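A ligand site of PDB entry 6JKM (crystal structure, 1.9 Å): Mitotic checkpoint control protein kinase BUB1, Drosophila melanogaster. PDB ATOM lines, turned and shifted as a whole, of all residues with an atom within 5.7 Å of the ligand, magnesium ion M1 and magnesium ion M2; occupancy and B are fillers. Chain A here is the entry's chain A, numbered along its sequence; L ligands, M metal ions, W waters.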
ATOM      1  N   ILE A  62     -13.046   8.002  11.610  1.00  0.00           N
ATOM      2  CA  ILE A  62     -14.328   8.002  10.866  1.00  0.00           C
ATOM      3  C   ILE A  62     -14.251   8.982   9.704  1.00  0.00           C
ATOM      4  O   ILE A  62     -14.469   8.604   8.560  1.00  0.00           O
ATOM      5  CB  ILE A  62     -15.527   8.376  11.748  1.00  0.00           C
ATOM      6  CG1 ILE A  62     -15.657   7.425  12.939  1.00  0.00           C
ATOM      7  CG2 ILE A  62     -16.815   8.419  10.898  1.00  0.00           C
ATOM      8  CD1 ILE A  62     -15.893   5.961  12.571  1.00  0.00           C
ATOM      9  N   GLY A  63     -13.931  10.240   9.996  1.00  0.00           N
ATOM     10  CA  GLY A  63     -13.703  11.226   8.952  1.00  0.00           C
ATOM     11  C   GLY A  63     -12.472  12.054   9.262  1.00  0.00           C
ATOM     12  O   GLY A  63     -12.124  12.250  10.434  1.00  0.00           O
ATOM     13  N   VAL A  70     -12.936  13.131  12.879  1.00  0.00           N
ATOM     14  CA  VAL A  70     -13.765  12.415  13.843  1.00  0.00           C
ATOM     15  C   VAL A  70     -13.227  10.990  13.996  1.00  0.00           C
ATOM     16  O   VAL A  70     -12.987  10.309  12.993  1.00  0.00           O
ATOM     17  CB  VAL A  70     -15.257  12.376  13.429  1.00  0.00           C
ATOM     18  CG1 VAL A  70     -16.052  11.525  14.397  1.00  0.00           C
ATOM     19  CG2 VAL A  70     -15.843  13.784  13.324  1.00  0.00           C
ATOM     20  N   ALA A  83     -17.714   9.293  20.197  1.00  0.00           N
ATOM     21  CA  ALA A  83     -17.103  10.015  19.082  1.00  0.00           C
ATOM     22  C   ALA A  83     -16.128  11.034  19.658  1.00  0.00           C
ATOM     23  O   ALA A  83     -16.425  11.671  20.672  1.00  0.00           O
ATOM     24  CB  ALA A  83     -18.140  10.705  18.225  1.00  0.00           C
ATOM     25  N   LYS A  85     -14.265  14.430  18.412  1.00  0.00           N
ATOM     26  CA  LYS A  85     -14.244  15.373  17.304  1.00  0.00           C
ATOM     27  C   LYS A  85     -13.170  16.409  17.548  1.00  0.00           C
ATOM     28  O   LYS A  85     -13.218  17.151  18.526  1.00  0.00           O
ATOM     29  CB  LYS A  85     -15.616  16.039  17.113  1.00  0.00           C
ATOM     30  CG  LYS A  85     -15.664  16.997  15.925  1.00  0.00           C
ATOM     31  CD  LYS A  85     -17.090  17.582  15.760  1.00  0.00           C
ATOM     32  CE  LYS A  85     -17.163  18.493  14.538  1.00  0.00           C
ATOM     33  NZ  LYS A  85     -18.581  18.812  14.166  1.00  0.00           N
ATOM     34  N   GLU A  87     -10.857  19.662  16.062  1.00  0.00           N
ATOM     35  CA  GLU A  87     -10.862  20.758  15.099  1.00  0.00           C
ATOM     36  C   GLU A  87      -9.753  21.764  15.397  1.00  0.00           C
ATOM     37  O   GLU A  87      -9.492  22.063  16.550  1.00  0.00           O
ATOM     38  CB  GLU A  87     -12.226  21.483  15.109  1.00  0.00           C
ATOM     39  CG  GLU A  87     -12.289  22.648  14.115  1.00  0.00           C
ATOM     40  CD  GLU A  87     -13.697  23.057  13.723  1.00  0.00           C
ATOM     41  OE1 GLU A  87     -14.675  22.357  14.109  1.00  0.00           O
ATOM     42  OE2 GLU A  87     -13.842  24.092  13.020  1.00  0.00           O
ATOM     43  N   GLU A  94     -18.917  26.033  18.667  1.00  0.00           N
ATOM     44  CA  GLU A  94     -19.650  24.775  18.657  1.00  0.00           C
ATOM     45  C   GLU A  94     -20.010  24.333  20.068  1.00  0.00           C
ATOM     46  O   GLU A  94     -21.117  23.883  20.324  1.00  0.00           O
ATOM     47  CB  GLU A  94     -18.832  23.674  17.962  1.00  0.00           C
ATOM     48  CG  GLU A  94     -19.529  22.326  17.907  1.00  0.00           C
ATOM     49  CD  GLU A  94     -18.972  21.464  16.785  1.00  0.00           C
ATOM     50  OE1 GLU A  94     -18.007  21.913  16.125  1.00  0.00           O
ATOM     51  OE2 GLU A  94     -19.487  20.346  16.562  1.00  0.00           O
ATOM     52  N   SER A 131     -18.510  12.821  22.639  1.00  0.00           N
ATOM     53  CA  SER A 131     -19.951  12.625  22.795  1.00  0.00           C
ATOM     54  C   SER A 131     -20.315  11.170  22.531  1.00  0.00           C
ATOM     55  O   SER A 131     -19.497  10.394  22.057  1.00  0.00           O
ATOM     56  CB  SER A 131     -20.717  13.548  21.839  1.00  0.00           C
ATOM     57  OG  SER A 131     -20.251  13.341  20.512  1.00  0.00           O
ATOM     58  N   GLU A 132     -21.562  10.803  22.839  1.00  0.00           N
ATOM     59  CA  GLU A 132     -22.043   9.446  22.605  1.00  0.00           C
ATOM     60  C   GLU A 132     -21.927   9.067  21.113  1.00  0.00           C
ATOM     61  O   GLU A 132     -22.346   9.822  20.228  1.00  0.00           O
ATOM     62  CB  GLU A 132     -23.500   9.310  23.076  1.00  0.00           C
ATOM     63  CG  GLU A 132     -24.045   7.910  22.885  1.00  0.00           C
ATOM     64  CD  GLU A 132     -25.535   7.788  23.209  1.00  0.00           C
ATOM     65  OE1 GLU A 132     -26.134   8.749  23.720  1.00  0.00           O
ATOM     66  OE2 GLU A 132     -26.105   6.706  22.925  1.00  0.00           O
ATOM     67  N   PHE A 133     -21.345   7.892  20.854  1.00  0.00           N
ATOM     68  CA  PHE A 133     -21.220   7.353  19.501  1.00  0.00           C
ATOM     69  C   PHE A 133     -22.482   6.606  19.074  1.00  0.00           C
ATOM     70  O   PHE A 133     -22.993   5.766  19.819  1.00  0.00           O
ATOM     71  CB  PHE A 133     -20.016   6.409  19.440  1.00  0.00           C
ATOM     72  CG  PHE A 133     -19.708   5.881  18.046  1.00  0.00           C
ATOM     73  CD1 PHE A 133     -19.055   6.670  17.116  1.00  0.00           C
ATOM     74  CD2 PHE A 133     -20.070   4.593  17.687  1.00  0.00           C
ATOM     75  CE1 PHE A 133     -18.756   6.189  15.868  1.00  0.00           C
ATOM     76  CE2 PHE A 133     -19.768   4.108  16.430  1.00  0.00           C
ATOM     77  CZ  PHE A 133     -19.111   4.906  15.521  1.00  0.00           C
ATOM     78  N   SER A 134     -22.975   6.869  17.867  1.00  0.00           N
ATOM     79  CA  SER A 134     -24.061   6.052  17.307  1.00  0.00           C
ATOM     80  C   SER A 134     -23.529   4.925  16.420  1.00  0.00           C
ATOM     81  O   SER A 134     -22.826   5.174  15.453  1.00  0.00           O
ATOM     82  CB  SER A 134     -25.011   6.915  16.487  1.00  0.00           C
ATOM     83  OG  SER A 134     -25.849   6.075  15.706  1.00  0.00           O
ATOM     84  N   ASP A 135     -23.892   3.678  16.707  1.00  0.00           N
ATOM     85  CA  ASP A 135     -23.437   2.574  15.868  1.00  0.00           C
ATOM     86  C   ASP A 135     -24.144   2.539  14.502  1.00  0.00           C
ATOM     87  O   ASP A 135     -23.756   1.764  13.610  1.00  0.00           O
ATOM     88  CB  ASP A 135     -23.633   1.236  16.567  1.00  0.00           C
ATOM     89  CG  ASP A 135     -22.668   1.022  17.711  1.00  0.00           C
ATOM     90  OD1 ASP A 135     -21.504   0.621  17.447  1.00  0.00           O
ATOM     91  OD2 ASP A 135     -23.071   1.254  18.869  1.00  0.00           O
ATOM     92  N   GLY A 137     -24.765   5.458  12.697  1.00  0.00           N
ATOM     93  CA  GLY A 137     -24.200   6.506  11.867  1.00  0.00           C
ATOM     94  C   GLY A 137     -25.212   7.527  11.401  1.00  0.00           C
ATOM     95  O   GLY A 137     -26.273   7.663  11.981  1.00  0.00           O
ATOM     96  N   SER A 138     -24.899   8.270  10.350  1.00  0.00           N
ATOM     97  CA  SER A 138     -25.772   9.356   9.910  1.00  0.00           C
ATOM     98  C   SER A 138     -26.837   8.847   8.953  1.00  0.00           C
ATOM     99  O   SER A 138     -26.808   7.695   8.497  1.00  0.00           O
ATOM    100  CB  SER A 138     -24.965  10.458   9.216  1.00  0.00           C
ATOM    101  OG  SER A 138     -24.540  10.016   7.932  1.00  0.00           O
ATOM    102  N   ASP A 182     -27.051  24.181   9.230  1.00  0.00           N
ATOM    103  CA  ASP A 182     -26.352  23.194   8.415  1.00  0.00           C
ATOM    104  C   ASP A 182     -27.161  21.889   8.411  1.00  0.00           C
ATOM    105  O   ASP A 182     -26.607  20.797   8.555  1.00  0.00           O
ATOM    106  CB  ASP A 182     -24.933  22.972   8.949  1.00  0.00           C
ATOM    107  CG  ASP A 182     -23.983  22.380   7.902  1.00  0.00           C
ATOM    108  OD1 ASP A 182     -24.293  22.422   6.696  1.00  0.00           O
ATOM    109  OD2 ASP A 182     -22.889  21.884   8.283  1.00  0.00           O
ATOM    110  N   LYS A 184     -28.521  18.862   7.056  1.00  0.00           N
ATOM    111  CA  LYS A 184     -28.341  17.964   5.930  1.00  0.00           C
ATOM    112  C   LYS A 184     -28.312  16.540   6.470  1.00  0.00           C
ATOM    113  O   LYS A 184     -28.220  16.364   7.687  1.00  0.00           O
ATOM    114  CB  LYS A 184     -27.080  18.311   5.137  1.00  0.00           C
ATOM    115  CG  LYS A 184     -25.807  18.435   5.921  1.00  0.00           C
ATOM    116  CD  LYS A 184     -24.681  18.750   4.915  1.00  0.00           C
ATOM    117  CE  LYS A 184     -23.587  19.617   5.492  1.00  0.00           C
ATOM    118  NZ  LYS A 184     -22.632  20.096   4.421  1.00  0.00           N
ATOM    119  N   ASP A 186     -26.192  14.298   6.632  1.00  0.00           N
ATOM    120  CA  ASP A 186     -24.927  14.088   7.339  1.00  0.00           C
ATOM    121  C   ASP A 186     -25.036  14.442   8.821  1.00  0.00           C
ATOM    122  O   ASP A 186     -24.338  13.867   9.661  1.00  0.00           O
ATOM    123  CB  ASP A 186     -23.805  14.966   6.717  1.00  0.00           C
ATOM    124  CG  ASP A 186     -23.769  14.903   5.195  1.00  0.00           C
ATOM    125  OD1 ASP A 186     -22.764  14.378   4.657  1.00  0.00           O
ATOM    126  OD2 ASP A 186     -24.780  15.302   4.554  1.00  0.00           O
ATOM    127  N   ASN A 187     -25.878  15.416   9.148  1.00  0.00           N
ATOM    128  CA  ASN A 187     -25.892  15.897  10.521  1.00  0.00           C
ATOM    129  C   ASN A 187     -27.078  15.414  11.363  1.00  0.00           C
ATOM    130  O   ASN A 187     -27.316  15.940  12.435  1.00  0.00           O
ATOM    131  CB  ASN A 187     -25.839  17.427  10.526  1.00  0.00           C
ATOM    132  CG  ASN A 187     -24.489  17.950  10.046  1.00  0.00           C
ATOM    133  OD1 ASN A 187     -23.455  17.280  10.221  1.00  0.00           O
ATOM    134  ND2 ASN A 187     -24.475  19.125   9.412  1.00  0.00           N
ATOM    135  N   LEU A 189     -28.068  11.794  13.124  1.00  0.00           N
ATOM    136  CA  LEU A 189     -27.669  10.431  13.436  1.00  0.00           C
ATOM    137  C   LEU A 189     -28.897   9.593  13.749  1.00  0.00           C
ATOM    138  O   LEU A 189     -29.847  10.106  14.328  1.00  0.00           O
ATOM    139  CB  LEU A 189     -26.730  10.394  14.651  1.00  0.00           C
ATOM    140  CG  LEU A 189     -25.347  11.055  14.536  1.00  0.00           C
ATOM    141  CD1 LEU A 189     -24.585  10.854  15.839  1.00  0.00           C
ATOM    142  CD2 LEU A 189     -24.573  10.527  13.338  1.00  0.00           C
ATOM    143  N   GLN A 204     -30.911  12.081  16.185  1.00  0.00           N
ATOM    144  CA  GLN A 204     -30.193  13.105  16.940  1.00  0.00           C
ATOM    145  C   GLN A 204     -29.547  14.087  15.981  1.00  0.00           C
ATOM    146  O   GLN A 204     -28.867  13.688  15.018  1.00  0.00           O
ATOM    147  CB  GLN A 204     -29.133  12.497  17.861  1.00  0.00           C
ATOM    148  CG  GLN A 204     -28.370  13.499  18.715  1.00  0.00           C
ATOM    149  CD  GLN A 204     -27.302  12.836  19.548  1.00  0.00           C
ATOM    150  OE1 GLN A 204     -26.183  12.612  19.061  1.00  0.00           O
ATOM    151  NE2 GLN A 204     -27.638  12.476  20.780  1.00  0.00           N
ATOM    152  N   ILE A 206     -26.728  16.766  15.215  1.00  0.00           N
ATOM    153  CA  ILE A 206     -25.356  17.004  15.642  1.00  0.00           C
ATOM    154  C   ILE A 206     -24.739  18.142  14.837  1.00  0.00           C
ATOM    155  O   ILE A 206     -25.364  18.683  13.920  1.00  0.00           O
ATOM    156  CB  ILE A 206     -24.474  15.744  15.455  1.00  0.00           C
ATOM    157  CG1 ILE A 206     -24.288  15.437  13.966  1.00  0.00           C
ATOM    158  CG2 ILE A 206     -25.098  14.540  16.150  1.00  0.00           C
ATOM    159  CD1 ILE A 206     -23.176  14.407  13.680  1.00  0.00           C
ATOM    160  N   ASP A 207     -23.491  18.493  15.165  1.00  0.00           N
ATOM    161  CA  ASP A 207     -22.682  19.436  14.398  1.00  0.00           C
ATOM    162  C   ASP A 207     -23.275  20.832  14.428  1.00  0.00           C
ATOM    163  O   ASP A 207     -23.832  21.317  13.440  1.00  0.00           O
ATOM    164  CB  ASP A 207     -22.527  18.951  12.957  1.00  0.00           C
ATOM    165  CG  ASP A 207     -21.471  19.723  12.191  1.00  0.00           C
ATOM    166  OD1 ASP A 207     -21.323  19.494  10.960  1.00  0.00           O
ATOM    167  OD2 ASP A 207     -20.785  20.569  12.805  1.00  0.00           O
ATOM    168  N   GLY A 209     -21.548  23.499  14.609  1.00  0.00           N
ATOM    169  CA  GLY A 209     -20.394  24.342  14.296  1.00  0.00           C
ATOM    170  C   GLY A 209     -20.726  25.711  13.713  1.00  0.00           C
ATOM    171  O   GLY A 209     -20.021  26.692  13.985  1.00  0.00           O
ATOM    172  N   VAL A 210     -21.775  25.815  12.907  1.00  0.00           N
ATOM    173  CA  VAL A 210     -22.127  27.111  12.335  1.00  0.00           C
ATOM    174  C   VAL A 210     -23.533  27.592  12.745  1.00  0.00           C
ATOM    175  O   VAL A 210     -24.158  28.402  12.046  1.00  0.00           O
ATOM    176  CB  VAL A 210     -22.031  27.087  10.793  1.00  0.00           C
ATOM    177  CG1 VAL A 210     -20.572  26.791  10.373  1.00  0.00           C
ATOM    178  CG2 VAL A 210     -22.992  26.073  10.197  1.00  0.00           C
HETATM  179  P1  LIG L   1     -18.224  18.128  10.582  1.00  0.00           P
HETATM  180  O1  LIG L   1     -16.838  17.903  10.060  1.00  0.00           O
HETATM  181  O2  LIG L   1     -18.362  19.438  11.323  1.00  0.00           O
HETATM  182  O3  LIG L   1     -19.293  17.891   9.522  1.00  0.00           O
HETATM  183  P2  LIG L   1     -19.688  16.219  12.244  1.00  0.00           P
HETATM  184  O4  LIG L   1     -19.793  16.463  13.746  1.00  0.00           O
HETATM  185  O5  LIG L   1     -20.864  16.447  11.345  1.00  0.00           O
HETATM  186  O6  LIG L   1     -18.349  16.941  11.697  1.00  0.00           O
HETATM  187  O7  LIG L   1     -19.265  14.674  12.013  1.00  0.00           O
HETATM  188  C1  LIG L   1     -18.903  14.214  10.697  1.00  0.00           C
HETATM  189  C2  LIG L   1     -19.426  12.799  10.462  1.00  0.00           C
HETATM  190  O8  LIG L   1     -18.861  11.892  11.422  1.00  0.00           O
HETATM  191  C3  LIG L   1     -20.924  12.699  10.710  1.00  0.00           C
HETATM  192  O9  LIG L   1     -21.690  13.034   9.554  1.00  0.00           O
HETATM  193  C4  LIG L   1     -21.063  11.226  11.056  1.00  0.00           C
HETATM  194  O10 LIG L   1     -21.075  10.502   9.812  1.00  0.00           O
HETATM  195  C5  LIG L   1     -19.798  10.909  11.848  1.00  0.00           C
HETATM  196  N1  LIG L   1     -20.126  11.157  13.275  1.00  0.00           N
HETATM  197  C6  LIG L   1     -20.004  12.336  13.928  1.00  0.00           C
HETATM  198  N2  LIG L   1     -20.406  12.229  15.213  1.00  0.00           N
HETATM  199  C7  LIG L   1     -20.827  10.961  15.404  1.00  0.00           C
HETATM  200  C8  LIG L   1     -21.377  10.181  16.524  1.00  0.00           C
HETATM  201  N3  LIG L   1     -21.584  10.741  17.757  1.00  0.00           N
HETATM  202  N4  LIG L   1     -21.680   8.881  16.285  1.00  0.00           N
HETATM  203  C9  LIG L   1     -21.479   8.304  15.089  1.00  0.00           C
HETATM  204  N5  LIG L   1     -20.971   8.952  14.029  1.00  0.00           N
HETATM  205  C10 LIG L   1     -20.640  10.263  14.128  1.00  0.00           C
HETATM  206 MG    MG M   1     -21.398  17.636   9.868  1.00  0.00          MG
HETATM  207 MG    MG M   2     -19.686  21.047  10.914  1.00  0.00          MG
HETATM  208  O   HOH W   1     -21.698  18.643   8.315  1.00  0.00           O
HETATM  209  O   HOH W   2     -22.051  13.875  18.353  1.00  0.00           O
HETATM  210  O   HOH W   3     -21.887  22.722  10.622  1.00  0.00           O
HETATM  211  O   HOH W   4     -18.962  22.747  11.331  1.00  0.00           O
HETATM  212  O   HOH W   5     -20.109  15.006  16.067  1.00  0.00           O
HETATM  213  O   HOH W   6     -20.122   6.865  12.398  1.00  0.00           O
HETATM  214  O   HOH W   7     -18.306  17.777   6.795  1.00  0.00           O
HETATM  215  O   HOH W   8     -17.629  21.822  13.373  1.00  0.00           O
HETATM  216  O   HOH W   9     -22.052  10.747   7.394  1.00  0.00           O
HETATM  217  O   HOH W  10     -21.328  15.975   8.666  1.00  0.00           O
HETATM  218  O   HOH W  11     -19.626  21.042   8.991  1.00  0.00           O
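The side-chain amino group (NZ) of Lys 85 lies within salt-bridge range of an oxygen (O4) of the ligand, at 2.7 Å.
O of Glu 132 sits at hydrogen-bond distance from N3 of the ligand, 2.7 Å away.
An oxygen (O9) of the ligand is in hydrogen-bond range of the backbone carbonyl oxygen (O) of Asp 186.
A nitrogen (N4) of the ligand sits at hydrogen-bond distance from the backbone NH of Ser 134 (2.9 Å).
The backbone carbonyl oxygen of Asn 187 sits at hydrogen-bond distance from the backbone NH of Ile 206, 3.0 Å away.
The side-chain amide nitrogen (ND2) of Asn 187 is in hydrogen-bond range of the backbone carbonyl oxygen (O) of Asp 182, at 2.8 Å.
The side-chain amino group (NZ) of Lys 85 sits close to the side-chain carboxylate (OD2) of Asp 207 (3.1 Å).
NZ of Lys 85 lies within salt-bridge range of OE2 of Glu 94 (3.0 Å).
The side-chain hydroxyl (OG) of Ser 134 lies within hydrogen-bond range of the backbone NH (N) of Gly 137, 3.3 Å away.
The backbone NH of Ala 83 is in hydrogen-bond range of the backbone carbonyl oxygen of Ser 131, at 2.8 Å.
O of Val 70 is in hydrogen-bond range of N of Ile 62.
N of Val 70 is in hydrogen-bond range of O of Gly 63, at 2.7 Å.
Merely in contact with the ligand: Leu 189, Ala 83, Phe 133, Val 70, Ile 206 and Ser 138.
The nearest printed residue that does not touch the ligand is Ile 62 (4.0001 Å).
Within 4 Å of magnesium ion M1: Asn 187 and Asp 207.
The nearest printed residue that does not touch magnesium ion M1 is Asp 182 (4.8 Å).
Within 4 Å of magnesium ion M2: Asp 207.
Water W1 is bound to magnesium ion M1 (1.9 Å).
An oxygen (O5) of the ligand binds magnesium ion M1.
Magnesium ion M1 is bound by water W10, at 2.1 Å.
OD1 of Asn 187 is bound to magnesium ion M1 (2.1 Å).
An oxygen (O3) of the ligand binds magnesium ion M1, 2.1 Å away.
OD1 of Asp 207 is bound to magnesium ion M1, 2.2 Å away.
Magnesium ion M1 has six donor atoms within binding distance.
Magnesium ion M2 is bound by water W4, 1.9 Å away.
Water W11 is bound to magnesium ion M2 (1.9 Å).
Magnesium ion M2 is bound by an oxygen (O2) of the ligand.
The side-chain carboxylate (OD2) of Asp 207 binds magnesium ion M2.
OD1 of Asp 207 binds magnesium ion M2 (2.3 Å).
Magnesium ion M2 has five donor atoms within binding distance.
Slightly farther from magnesium ion M2 lies water W3 (2.8 Å).
Water W1 lies within hydrogen-bond range of ND2 of Asn 187 and OD2 of Asp 182.
Water W9 bridges an oxygen (O10) of the ligand (2.6 Å) and the side-chain hydroxyl (OG) of Ser 138 (2.6 Å).
Water W2 bridges the side-chain hydroxyl (OG) of Ser 131 (2.9 Å) and a nitrogen (N3) of the ligand (3.2 Å).
Water W8 lies within hydrogen-bond range of OE1 of Glu 94, OE1 of Glu 87 and NZ of Lys 85.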
